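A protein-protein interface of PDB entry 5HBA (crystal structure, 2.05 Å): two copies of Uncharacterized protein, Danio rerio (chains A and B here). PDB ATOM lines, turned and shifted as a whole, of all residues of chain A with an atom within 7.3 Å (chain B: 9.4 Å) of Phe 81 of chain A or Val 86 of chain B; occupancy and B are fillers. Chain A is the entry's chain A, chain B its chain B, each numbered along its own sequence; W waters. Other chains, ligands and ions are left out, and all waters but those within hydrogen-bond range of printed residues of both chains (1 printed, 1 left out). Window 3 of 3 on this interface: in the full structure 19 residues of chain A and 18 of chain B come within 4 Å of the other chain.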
ATOM      1  N   GLY A  60     -37.058 -16.216   6.720  1.00  0.00           N
ATOM      2  CA  GLY A  60     -36.267 -15.953   5.531  1.00  0.00           C
ATOM      3  C   GLY A  60     -34.920 -15.332   5.859  1.00  0.00           C
ATOM      4  O   GLY A  60     -34.451 -15.419   6.997  1.00  0.00           O
ATOM      5  N   ARG A  61     -34.304 -14.699   4.862  1.00  0.00           N
ATOM      6  CA  ARG A  61     -32.979 -14.097   5.013  1.00  0.00           C
ATOM      7  C   ARG A  61     -32.931 -13.083   6.164  1.00  0.00           C
ATOM      8  O   ARG A  61     -33.799 -12.210   6.273  1.00  0.00           O
ATOM      9  CB  ARG A  61     -32.553 -13.418   3.704  1.00  0.00           C
ATOM     10  CG  ARG A  61     -31.138 -12.837   3.734  1.00  0.00           C
ATOM     11  CD  ARG A  61     -31.088 -11.440   3.125  1.00  0.00           C
ATOM     12  NE  ARG A  61     -31.951 -10.520   3.852  1.00  0.00           N
ATOM     13  CZ  ARG A  61     -32.877  -9.748   3.286  1.00  0.00           C
ATOM     14  NH1 ARG A  61     -33.629  -8.955   4.046  1.00  0.00           N
ATOM     15  NH2 ARG A  61     -33.052  -9.767   1.968  1.00  0.00           N
ATOM     16  N   LEU A  62     -31.923 -13.215   7.025  1.00  0.00           N
ATOM     17  CA  LEU A  62     -31.729 -12.287   8.138  1.00  0.00           C
ATOM     18  C   LEU A  62     -30.299 -11.776   8.169  1.00  0.00           C
ATOM     19  O   LEU A  62     -29.349 -12.557   8.304  1.00  0.00           O
ATOM     20  CB  LEU A  62     -32.082 -12.926   9.490  1.00  0.00           C
ATOM     21  CG  LEU A  62     -31.827 -12.033  10.720  1.00  0.00           C
ATOM     22  CD1 LEU A  62     -32.537 -10.679  10.616  1.00  0.00           C
ATOM     23  CD2 LEU A  62     -32.245 -12.741  11.999  1.00  0.00           C
ATOM     24  N   CYS A  63     -30.164 -10.461   8.027  1.00  0.00           N
ATOM     25  CA  CYS A  63     -28.879  -9.790   8.133  1.00  0.00           C
ATOM     26  C   CYS A  63     -28.956  -8.736   9.242  1.00  0.00           C
ATOM     27  O   CYS A  63     -29.889  -7.924   9.277  1.00  0.00           O
ATOM     28  CB  CYS A  63     -28.527  -9.119   6.810  1.00  0.00           C
ATOM     29  SG  CYS A  63     -27.791 -10.228   5.587  1.00  0.00           S
ATOM     30  N   PHE A  78     -23.552  -9.846  10.204  1.00  0.00           N
ATOM     31  CA  PHE A  78     -23.786 -11.262  10.428  1.00  0.00           C
ATOM     32  C   PHE A  78     -25.041 -11.626   9.662  1.00  0.00           C
ATOM     33  O   PHE A  78     -26.111 -11.108   9.965  1.00  0.00           O
ATOM     34  CB  PHE A  78     -23.968 -11.536  11.926  1.00  0.00           C
ATOM     35  CG  PHE A  78     -22.788 -11.110  12.757  1.00  0.00           C
ATOM     36  CD1 PHE A  78     -21.691 -11.956  12.927  1.00  0.00           C
ATOM     37  CD2 PHE A  78     -22.754  -9.851  13.336  1.00  0.00           C
ATOM     38  CE1 PHE A  78     -20.581 -11.543  13.682  1.00  0.00           C
ATOM     39  CE2 PHE A  78     -21.657  -9.436  14.094  1.00  0.00           C
ATOM     40  CZ  PHE A  78     -20.573 -10.282  14.263  1.00  0.00           C
ATOM     41  N   CYS A  79     -24.893 -12.499   8.665  1.00  0.00           N
ATOM     42  CA  CYS A  79     -25.964 -12.808   7.715  1.00  0.00           C
ATOM     43  C   CYS A  79     -26.248 -14.312   7.574  1.00  0.00           C
ATOM     44  O   CYS A  79     -25.330 -15.119   7.352  1.00  0.00           O
ATOM     45  CB  CYS A  79     -25.600 -12.274   6.320  1.00  0.00           C
ATOM     46  SG  CYS A  79     -25.792 -10.509   6.017  1.00  0.00           S
ATOM     47  N   ASP A  80     -27.524 -14.675   7.689  1.00  0.00           N
ATOM     48  CA  ASP A  80     -28.001 -15.991   7.260  1.00  0.00           C
ATOM     49  C   ASP A  80     -28.748 -15.809   5.938  1.00  0.00           C
ATOM     50  O   ASP A  80     -29.847 -15.241   5.918  1.00  0.00           O
ATOM     51  CB  ASP A  80     -28.954 -16.599   8.295  1.00  0.00           C
ATOM     52  CG  ASP A  80     -28.228 -17.364   9.404  1.00  0.00           C
ATOM     53  OD1 ASP A  80     -26.985 -17.377   9.407  1.00  0.00           O
ATOM     54  OD2 ASP A  80     -28.910 -17.932  10.292  1.00  0.00           O
ATOM     55  N   PHE A  81     -28.152 -16.280   4.845  1.00  0.00           N
ATOM     56  CA  PHE A  81     -28.791 -16.215   3.530  1.00  0.00           C
ATOM     57  C   PHE A  81     -29.550 -17.505   3.204  1.00  0.00           C
ATOM     58  O   PHE A  81     -29.272 -18.158   2.198  1.00  0.00           O
ATOM     59  CB  PHE A  81     -27.755 -15.925   2.432  1.00  0.00           C
ATOM     60  CG  PHE A  81     -27.240 -14.514   2.437  1.00  0.00           C
ATOM     61  CD1 PHE A  81     -27.999 -13.484   1.899  1.00  0.00           C
ATOM     62  CD2 PHE A  81     -25.993 -14.219   2.965  1.00  0.00           C
ATOM     63  CE1 PHE A  81     -27.525 -12.177   1.898  1.00  0.00           C
ATOM     64  CE2 PHE A  81     -25.509 -12.921   2.969  1.00  0.00           C
ATOM     65  CZ  PHE A  81     -26.281 -11.893   2.438  1.00  0.00           C
ATOM     66  N   ASN A  82     -30.511 -17.861   4.054  1.00  0.00           N
ATOM     67  CA  ASN A  82     -31.326 -19.051   3.832  1.00  0.00           C
ATOM     68  C   ASN A  82     -32.578 -18.757   3.009  1.00  0.00           C
ATOM     69  O   ASN A  82     -32.829 -17.607   2.625  1.00  0.00           O
ATOM     70  CB  ASN A  82     -31.716 -19.705   5.164  1.00  0.00           C
ATOM     71  CG  ASN A  82     -32.428 -18.745   6.101  1.00  0.00           C
ATOM     72  OD1 ASN A  82     -31.797 -18.086   6.932  1.00  0.00           O
ATOM     73  ND2 ASN A  82     -33.753 -18.670   5.983  1.00  0.00           N
ATOM     74  N   SER A  83     -33.358 -19.806   2.751  1.00  0.00           N
ATOM     75  CA  SER A  83     -34.575 -19.709   1.944  1.00  0.00           C
ATOM     76  C   SER A  83     -35.726 -19.007   2.679  1.00  0.00           C
ATOM     77  O   SER A  83     -35.750 -18.945   3.913  1.00  0.00           O
ATOM     78  CB  SER A  83     -35.035 -21.100   1.504  1.00  0.00           C
ATOM     79  OG  SER A  83     -35.947 -21.643   2.442  1.00  0.00           O
ATOM     80  N   LEU A  88     -34.095 -19.056  11.002  1.00  0.00           N
ATOM     81  CA  LEU A  88     -32.896 -19.501  11.721  1.00  0.00           C
ATOM     82  C   LEU A  88     -32.444 -18.450  12.743  1.00  0.00           C
ATOM     83  O   LEU A  88     -32.851 -17.290  12.665  1.00  0.00           O
ATOM     84  CB  LEU A  88     -31.754 -19.770  10.737  1.00  0.00           C
ATOM     85  CG  LEU A  88     -31.981 -20.782   9.609  1.00  0.00           C
ATOM     86  CD1 LEU A  88     -30.755 -20.877   8.689  1.00  0.00           C
ATOM     87  CD2 LEU A  88     -32.324 -22.143  10.188  1.00  0.00           C
ATOM     88  N   VAL A  90     -29.517 -16.174  13.947  1.00  0.00           N
ATOM     89  CA  VAL A  90     -28.204 -15.612  13.667  1.00  0.00           C
ATOM     90  C   VAL A  90     -27.658 -15.031  14.962  1.00  0.00           C
ATOM     91  O   VAL A  90     -28.357 -14.312  15.671  1.00  0.00           O
ATOM     92  CB  VAL A  90     -28.263 -14.452  12.657  1.00  0.00           C
ATOM     93  CG1 VAL A  90     -26.847 -14.041  12.244  1.00  0.00           C
ATOM     94  CG2 VAL A  90     -29.062 -14.832  11.444  1.00  0.00           C
ATOM     95  N   PHE A 109     -30.574  -5.198   8.077  1.00  0.00           N
ATOM     96  CA  PHE A 109     -30.502  -4.704   6.703  1.00  0.00           C
ATOM     97  C   PHE A 109     -30.906  -5.804   5.716  1.00  0.00           C
ATOM     98  O   PHE A 109     -30.996  -6.975   6.089  1.00  0.00           O
ATOM     99  CB  PHE A 109     -29.122  -4.113   6.378  1.00  0.00           C
ATOM    100  CG  PHE A 109     -27.986  -5.111   6.375  1.00  0.00           C
ATOM    101  CD1 PHE A 109     -27.413  -5.545   7.566  1.00  0.00           C
ATOM    102  CD2 PHE A 109     -27.438  -5.557   5.169  1.00  0.00           C
ATOM    103  CE1 PHE A 109     -26.345  -6.445   7.556  1.00  0.00           C
ATOM    104  CE2 PHE A 109     -26.357  -6.448   5.148  1.00  0.00           C
ATOM    105  CZ  PHE A 109     -25.814  -6.896   6.340  1.00  0.00           C
ATOM    106  N   ALA A 110     -31.211  -5.422   4.481  1.00  0.00           N
ATOM    107  CA  ALA A 110     -31.514  -6.405   3.449  1.00  0.00           C
ATOM    108  C   ALA A 110     -30.225  -6.716   2.690  1.00  0.00           C
ATOM    109  O   ALA A 110     -29.807  -5.962   1.805  1.00  0.00           O
ATOM    110  CB  ALA A 110     -32.588  -5.897   2.507  1.00  0.00           C
ATOM    111  N   GLY A 111     -29.595  -7.826   3.064  1.00  0.00           N
ATOM    112  CA  GLY A 111     -28.313  -8.230   2.511  1.00  0.00           C
ATOM    113  C   GLY A 111     -28.286  -8.516   1.022  1.00  0.00           C
ATOM    114  O   GLY A 111     -27.214  -8.589   0.429  1.00  0.00           O
ATOM    115  N   ASP A 112     -29.451  -8.703   0.413  1.00  0.00           N
ATOM    116  CA  ASP A 112     -29.523  -8.836  -1.041  1.00  0.00           C
ATOM    117  C   ASP A 112     -30.915  -8.421  -1.534  1.00  0.00           C
ATOM    118  O   ASP A 112     -31.728  -7.915  -0.752  1.00  0.00           O
ATOM    119  CB  ASP A 112     -29.140 -10.260  -1.499  1.00  0.00           C
ATOM    120  CG  ASP A 112     -30.115 -11.334  -1.004  1.00  0.00           C
ATOM    121  OD1 ASP A 112     -31.026 -11.013  -0.207  1.00  0.00           O
ATOM    122  OD2 ASP A 112     -29.964 -12.515  -1.406  1.00  0.00           O
ATOM    123  N   GLY A 113     -31.186  -8.623  -2.823  1.00  0.00           N
ATOM    124  CA  GLY A 113     -32.479  -8.261  -3.382  1.00  0.00           C
ATOM    125  C   GLY A 113     -32.539  -6.782  -3.723  1.00  0.00           C
ATOM    126  O   GLY A 113     -31.597  -6.034  -3.448  1.00  0.00           O
ATOM    127  N   SER B  57     -18.832 -17.015   8.985  1.00  0.00           N
ATOM    128  CA  SER B  57     -19.666 -17.414   7.862  1.00  0.00           C
ATOM    129  C   SER B  57     -18.833 -17.707   6.628  1.00  0.00           C
ATOM    130  O   SER B  57     -17.795 -17.086   6.379  1.00  0.00           O
ATOM    131  CB  SER B  57     -20.758 -16.375   7.557  1.00  0.00           C
ATOM    132  OG  SER B  57     -20.217 -15.090   7.294  1.00  0.00           O
ATOM    133  N   SER B  58     -19.308 -18.669   5.862  1.00  0.00           N
ATOM    134  CA  SER B  58     -18.663 -19.067   4.632  1.00  0.00           C
ATOM    135  C   SER B  58     -19.753 -19.653   3.759  1.00  0.00           C
ATOM    136  O   SER B  58     -20.803 -20.080   4.262  1.00  0.00           O
ATOM    137  CB  SER B  58     -17.582 -20.105   4.923  1.00  0.00           C
ATOM    138  OG  SER B  58     -17.219 -20.800   3.749  1.00  0.00           O
ATOM    139  N   GLU B  59     -19.515 -19.662   2.456  1.00  0.00           N
ATOM    140  CA  GLU B  59     -20.490 -20.193   1.520  1.00  0.00           C
ATOM    141  C   GLU B  59     -20.498 -21.717   1.625  1.00  0.00           C
ATOM    142  O   GLU B  59     -19.447 -22.342   1.755  1.00  0.00           O
ATOM    143  CB  GLU B  59     -20.154 -19.737   0.101  1.00  0.00           C
ATOM    144  CG  GLU B  59     -21.365 -19.464  -0.770  1.00  0.00           C
ATOM    145  CD  GLU B  59     -20.980 -19.118  -2.195  1.00  0.00           C
ATOM    146  OE1 GLU B  59     -19.776 -19.225  -2.527  1.00  0.00           O
ATOM    147  OE2 GLU B  59     -21.875 -18.743  -2.984  1.00  0.00           O
ATOM    148  N   GLY B  60     -21.687 -22.308   1.599  1.00  0.00           N
ATOM    149  CA  GLY B  60     -21.822 -23.745   1.735  1.00  0.00           C
ATOM    150  C   GLY B  60     -21.473 -24.247   3.126  1.00  0.00           C
ATOM    151  O   GLY B  60     -21.548 -23.503   4.111  1.00  0.00           O
ATOM    152  N   ARG B  61     -21.102 -25.521   3.195  1.00  0.00           N
ATOM    153  CA  ARG B  61     -20.692 -26.181   4.430  1.00  0.00           C
ATOM    154  C   ARG B  61     -19.569 -25.435   5.168  1.00  0.00           C
ATOM    155  O   ARG B  61     -18.579 -25.019   4.550  1.00  0.00           O
ATOM    156  CB  ARG B  61     -20.219 -27.581   4.069  1.00  0.00           C
ATOM    157  CG  ARG B  61     -20.029 -28.542   5.214  1.00  0.00           C
ATOM    158  CD  ARG B  61     -20.449 -29.916   4.720  1.00  0.00           C
ATOM    159  NE  ARG B  61     -19.525 -30.984   5.083  1.00  0.00           N
ATOM    160  CZ  ARG B  61     -19.666 -32.246   4.689  1.00  0.00           C
ATOM    161  NH1 ARG B  61     -20.694 -32.592   3.920  1.00  0.00           N
ATOM    162  NH2 ARG B  61     -18.785 -33.162   5.062  1.00  0.00           N
ATOM    163  N   LEU B  62     -19.731 -25.269   6.483  1.00  0.00           N
ATOM    164  CA  LEU B  62     -18.697 -24.664   7.317  1.00  0.00           C
ATOM    165  C   LEU B  62     -18.533 -25.404   8.640  1.00  0.00           C
ATOM    166  O   LEU B  62     -19.464 -25.466   9.448  1.00  0.00           O
ATOM    167  CB  LEU B  62     -19.003 -23.182   7.587  1.00  0.00           C
ATOM    168  CG  LEU B  62     -18.016 -22.500   8.536  1.00  0.00           C
ATOM    169  CD1 LEU B  62     -16.571 -22.704   8.063  1.00  0.00           C
ATOM    170  CD2 LEU B  62     -18.322 -21.014   8.667  1.00  0.00           C
ATOM    171  N   ASP B  80     -22.051 -26.218  10.431  1.00  0.00           N
ATOM    172  CA  ASP B  80     -23.281 -25.927   9.700  1.00  0.00           C
ATOM    173  C   ASP B  80     -23.248 -26.754   8.414  1.00  0.00           C
ATOM    174  O   ASP B  80     -22.468 -26.461   7.507  1.00  0.00           O
ATOM    175  CB  ASP B  80     -23.378 -24.433   9.363  1.00  0.00           C
ATOM    176  CG  ASP B  80     -24.131 -23.622  10.420  1.00  0.00           C
ATOM    177  OD1 ASP B  80     -24.510 -24.170  11.482  1.00  0.00           O
ATOM    178  OD2 ASP B  80     -24.352 -22.416  10.180  1.00  0.00           O
ATOM    179  N   PHE B  81     -24.067 -27.801   8.346  1.00  0.00           N
ATOM    180  CA  PHE B  81     -24.079 -28.664   7.163  1.00  0.00           C
ATOM    181  C   PHE B  81     -25.177 -28.232   6.202  1.00  0.00           C
ATOM    182  O   PHE B  81     -26.170 -28.938   6.032  1.00  0.00           O
ATOM    183  CB  PHE B  81     -24.272 -30.141   7.540  1.00  0.00           C
ATOM    184  CG  PHE B  81     -23.080 -30.766   8.217  1.00  0.00           C
ATOM    185  CD1 PHE B  81     -21.964 -31.147   7.482  1.00  0.00           C
ATOM    186  CD2 PHE B  81     -23.079 -30.993   9.584  1.00  0.00           C
ATOM    187  CE1 PHE B  81     -20.863 -31.728   8.099  1.00  0.00           C
ATOM    188  CE2 PHE B  81     -21.985 -31.583  10.209  1.00  0.00           C
ATOM    189  CZ  PHE B  81     -20.873 -31.946   9.463  1.00  0.00           C
ATOM    190  N   ASN B  82     -24.998 -27.072   5.579  1.00  0.00           N
ATOM    191  CA  ASN B  82     -25.983 -26.540   4.644  1.00  0.00           C
ATOM    192  C   ASN B  82     -25.553 -26.650   3.176  1.00  0.00           C
ATOM    193  O   ASN B  82     -24.406 -27.002   2.874  1.00  0.00           O
ATOM    194  CB  ASN B  82     -26.293 -25.081   4.984  1.00  0.00           C
ATOM    195  CG  ASN B  82     -25.060 -24.197   4.919  1.00  0.00           C
ATOM    196  OD1 ASN B  82     -24.426 -23.916   5.940  1.00  0.00           O
ATOM    197  ND2 ASN B  82     -24.709 -23.760   3.715  1.00  0.00           N
ATOM    198  N   SER B  83     -26.472 -26.310   2.271  1.00  0.00           N
ATOM    199  CA  SER B  83     -26.245 -26.426   0.824  1.00  0.00           C
ATOM    200  C   SER B  83     -25.267 -25.395   0.256  1.00  0.00           C
ATOM    201  O   SER B  83     -24.962 -24.383   0.896  1.00  0.00           O
ATOM    202  CB  SER B  83     -27.566 -26.303   0.065  1.00  0.00           C
ATOM    203  OG  SER B  83     -27.873 -24.939  -0.175  1.00  0.00           O
ATOM    204  N   LYS B  84     -24.824 -25.659  -0.974  1.00  0.00           N
ATOM    205  CA  LYS B  84     -23.779 -24.896  -1.665  1.00  0.00           C
ATOM    206  C   LYS B  84     -24.030 -23.391  -1.816  1.00  0.00           C
ATOM    207  O   LYS B  84     -23.101 -22.589  -1.707  1.00  0.00           O
ATOM    208  CB  LYS B  84     -23.525 -25.497  -3.062  1.00  0.00           C
ATOM    209  CG  LYS B  84     -24.759 -25.474  -3.984  1.00  0.00           C
ATOM    210  CD  LYS B  84     -24.407 -25.713  -5.456  1.00  0.00           C
ATOM    211  CE  LYS B  84     -25.610 -25.440  -6.363  1.00  0.00           C
ATOM    212  NZ  LYS B  84     -25.269 -25.511  -7.817  1.00  0.00           N
ATOM    213  N   SER B  85     -25.272 -23.009  -2.089  1.00  0.00           N
ATOM    214  CA  SER B  85     -25.570 -21.619  -2.432  1.00  0.00           C
ATOM    215  C   SER B  85     -25.910 -20.754  -1.215  1.00  0.00           C
ATOM    216  O   SER B  85     -26.315 -19.596  -1.359  1.00  0.00           O
ATOM    217  CB  SER B  85     -26.702 -21.560  -3.461  1.00  0.00           C
ATOM    218  OG  SER B  85     -27.733 -22.477  -3.134  1.00  0.00           O
ATOM    219  N   VAL B  86     -25.726 -21.310  -0.021  1.00  0.00           N
ATOM    220  CA  VAL B  86     -26.152 -20.636   1.200  1.00  0.00           C
ATOM    221  C   VAL B  86     -24.991 -20.308   2.145  1.00  0.00           C
ATOM    222  O   VAL B  86     -24.129 -21.150   2.418  1.00  0.00           O
ATOM    223  CB  VAL B  86     -27.219 -21.471   1.940  1.00  0.00           C
ATOM    224  CG1 VAL B  86     -27.685 -20.763   3.193  1.00  0.00           C
ATOM    225  CG2 VAL B  86     -28.399 -21.735   1.026  1.00  0.00           C
ATOM    226  N   SER B  87     -24.977 -19.069   2.631  1.00  0.00           N
ATOM    227  CA  SER B  87     -23.996 -18.624   3.611  1.00  0.00           C
ATOM    228  C   SER B  87     -24.696 -18.369   4.947  1.00  0.00           C
ATOM    229  O   SER B  87     -25.655 -17.597   5.015  1.00  0.00           O
ATOM    230  CB  SER B  87     -23.317 -17.350   3.120  1.00  0.00           C
ATOM    231  OG  SER B  87     -22.338 -16.923   4.043  1.00  0.00           O
ATOM    232  N   LEU B  88     -24.230 -19.033   5.999  1.00  0.00           N
ATOM    233  CA  LEU B  88     -24.840 -18.913   7.312  1.00  0.00           C
ATOM    234  C   LEU B  88     -23.769 -18.567   8.342  1.00  0.00           C
ATOM    235  O   LEU B  88     -22.588 -18.794   8.108  1.00  0.00           O
ATOM    236  CB  LEU B  88     -25.526 -20.227   7.705  1.00  0.00           C
ATOM    237  CG  LEU B  88     -26.625 -20.775   6.793  1.00  0.00           C
ATOM    238  CD1 LEU B  88     -27.168 -22.088   7.353  1.00  0.00           C
ATOM    239  CD2 LEU B  88     -27.755 -19.762   6.639  1.00  0.00           C
ATOM    240  N   VAL B  89     -24.182 -18.021   9.482  1.00  0.00           N
ATOM    241  CA  VAL B  89     -23.239 -17.722  10.560  1.00  0.00           C
ATOM    242  C   VAL B  89     -23.210 -18.856  11.581  1.00  0.00           C
ATOM    243  O   VAL B  89     -24.213 -19.114  12.247  1.00  0.00           O
ATOM    244  CB  VAL B  89     -23.612 -16.417  11.303  1.00  0.00           C
ATOM    245  CG1 VAL B  89     -22.617 -16.147  12.443  1.00  0.00           C
ATOM    246  CG2 VAL B  89     -23.669 -15.220  10.328  1.00  0.00           C
ATOM    247  N   LYS B 120     -12.537 -22.244   1.389  1.00  0.00           N
ATOM    248  CA  LYS B 120     -13.227 -21.035   0.942  1.00  0.00           C
ATOM    249  C   LYS B 120     -12.843 -19.842   1.803  1.00  0.00           C
ATOM    250  O   LYS B 120     -12.291 -20.011   2.899  1.00  0.00           O
ATOM    251  CB  LYS B 120     -14.741 -21.241   1.012  1.00  0.00           C
ATOM    252  CG  LYS B 120     -15.284 -22.217  -0.016  1.00  0.00           C
ATOM    253  CD  LYS B 120     -16.599 -22.833   0.432  1.00  0.00           C
ATOM    254  CE  LYS B 120     -16.392 -23.843   1.563  1.00  0.00           C
ATOM    255  NZ  LYS B 120     -17.674 -24.487   1.998  1.00  0.00           N
HETATM  256  O   HOH W   1     -22.064 -13.013   7.694  1.00  0.00           O
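The side-chain carboxylate (OD1) of Asp 80 of chain A is in hydrogen-bond range of the backbone NH (N) of Val 89 of chain B (2.9 Å). O of Ser 87 of chain B is in hydrogen-bond range of N of Phe 81 of chain A. O of Cys 79 of chain A sits close to O of Ser 87 of chain B (3.4 Å).
O of Leu 62 of chain A sits at hydrogen-bond distance from N of Asp 80 of chain A (2.9 Å). The side-chain sulfur (SG) of Cys 63 of chain A is disulfide-bonded to the side-chain sulfur (SG) of Cys 79 of chain A (2.1 Å). The backbone NH of Gly 60 of chain B lies within hydrogen-bond range of the backbone carbonyl oxygen of Val 86 of chain B, 2.8 Å away. The side-chain amide nitrogen (ND2) of Asn 82 of chain B sits at hydrogen-bond distance from the backbone carbonyl oxygen (O) of Val 86 of chain B.
Among the printed residues, merely in contact across the chains: Phe 78 of chain A with Val 89 of chain B, Cys 79 of chain A with Leu 88 of chain B, Cys 79 of chain A with Val 89 of chain B, Asp 80 of chain A with Ser 87 of chain B, Asp 80 of chain A with Leu 88 of chain B, Phe 81 of chain A with Val 86 of chain B, Phe 81 of chain A with Leu 88 of chain B, Leu 88 of chain A with Leu 88 of chain B and Val 90 of chain A with Val 89 of chain B.
Of chain B, only Val 86 (3.2 Å), Ser 87 (2.8 Å) and Leu 88 (3.9 Å) come within 4 Å of Phe 81 of chain A. Of the printed residues of chain A, Val 86 of chain B touches Phe 81 (3.2 Å). Asn 82 of chain A touches none of the printed residues of chain B. Of the printed residues of chain B, Leu 88 of chain A touches Leu 88. Printed residues of chain A within 4 Å of Ser 87 of chain B: Cys 79 (3.4 Å), Asp 80 (3.6 Å) and Phe 81 (2.8 Å). The nearest residue of chain B that does not touch Phe 81 of chain A is Ser 85 of chain B (4.8 Å). The nearest printed residue of chain B that does not touch Phe 78 of chain A is Ser 57 of chain B (6.1 Å).
Of the 17 printed residues of chain B, 4 touch a printed residue of chain A. Printed residues of chain B that touch a printed residue of chain A: Val 86, Ser 87, Leu 88 and Val 89. Hydrophobic or aromatic side chains of chain B that line the printed part of chain A: Val 86, Leu 88 and Val 89. Of the 17 printed residues of chain A, 6 touch a printed residue of chain B. Printed residues of chain A that touch a printed residue of chain B: Phe 78, Cys 79, Asp 80, Phe 81, Leu 88 and Val 90. Hydrophobic or aromatic side chains of chain A within 4 Å of the printed part of chain B: Phe 81, Leu 88 and Val 90. Among the printed residues, no Asp or Glu carboxylate lies within 4 Å of a Lys or Arg side-chain nitrogen of the other chain.
Asp 80 of chain A touches Leu 88 of chain B, but with the chains exchanged Leu 88 of chain A does not touch Asp 80 of chain B (6.8 Å). Phe 81 of chain A touches Leu 88 of chain B, but with the chains exchanged Leu 88 of chain A does not touch Phe 81 of chain B (9.6 Å). Leu 88 of chain B touches its own counterpart, Leu 88 of chain A.
Water W1 bridges the side-chain hydroxyl of Ser 57 of chain B and the backbone NH of Cys 79 of chain A.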
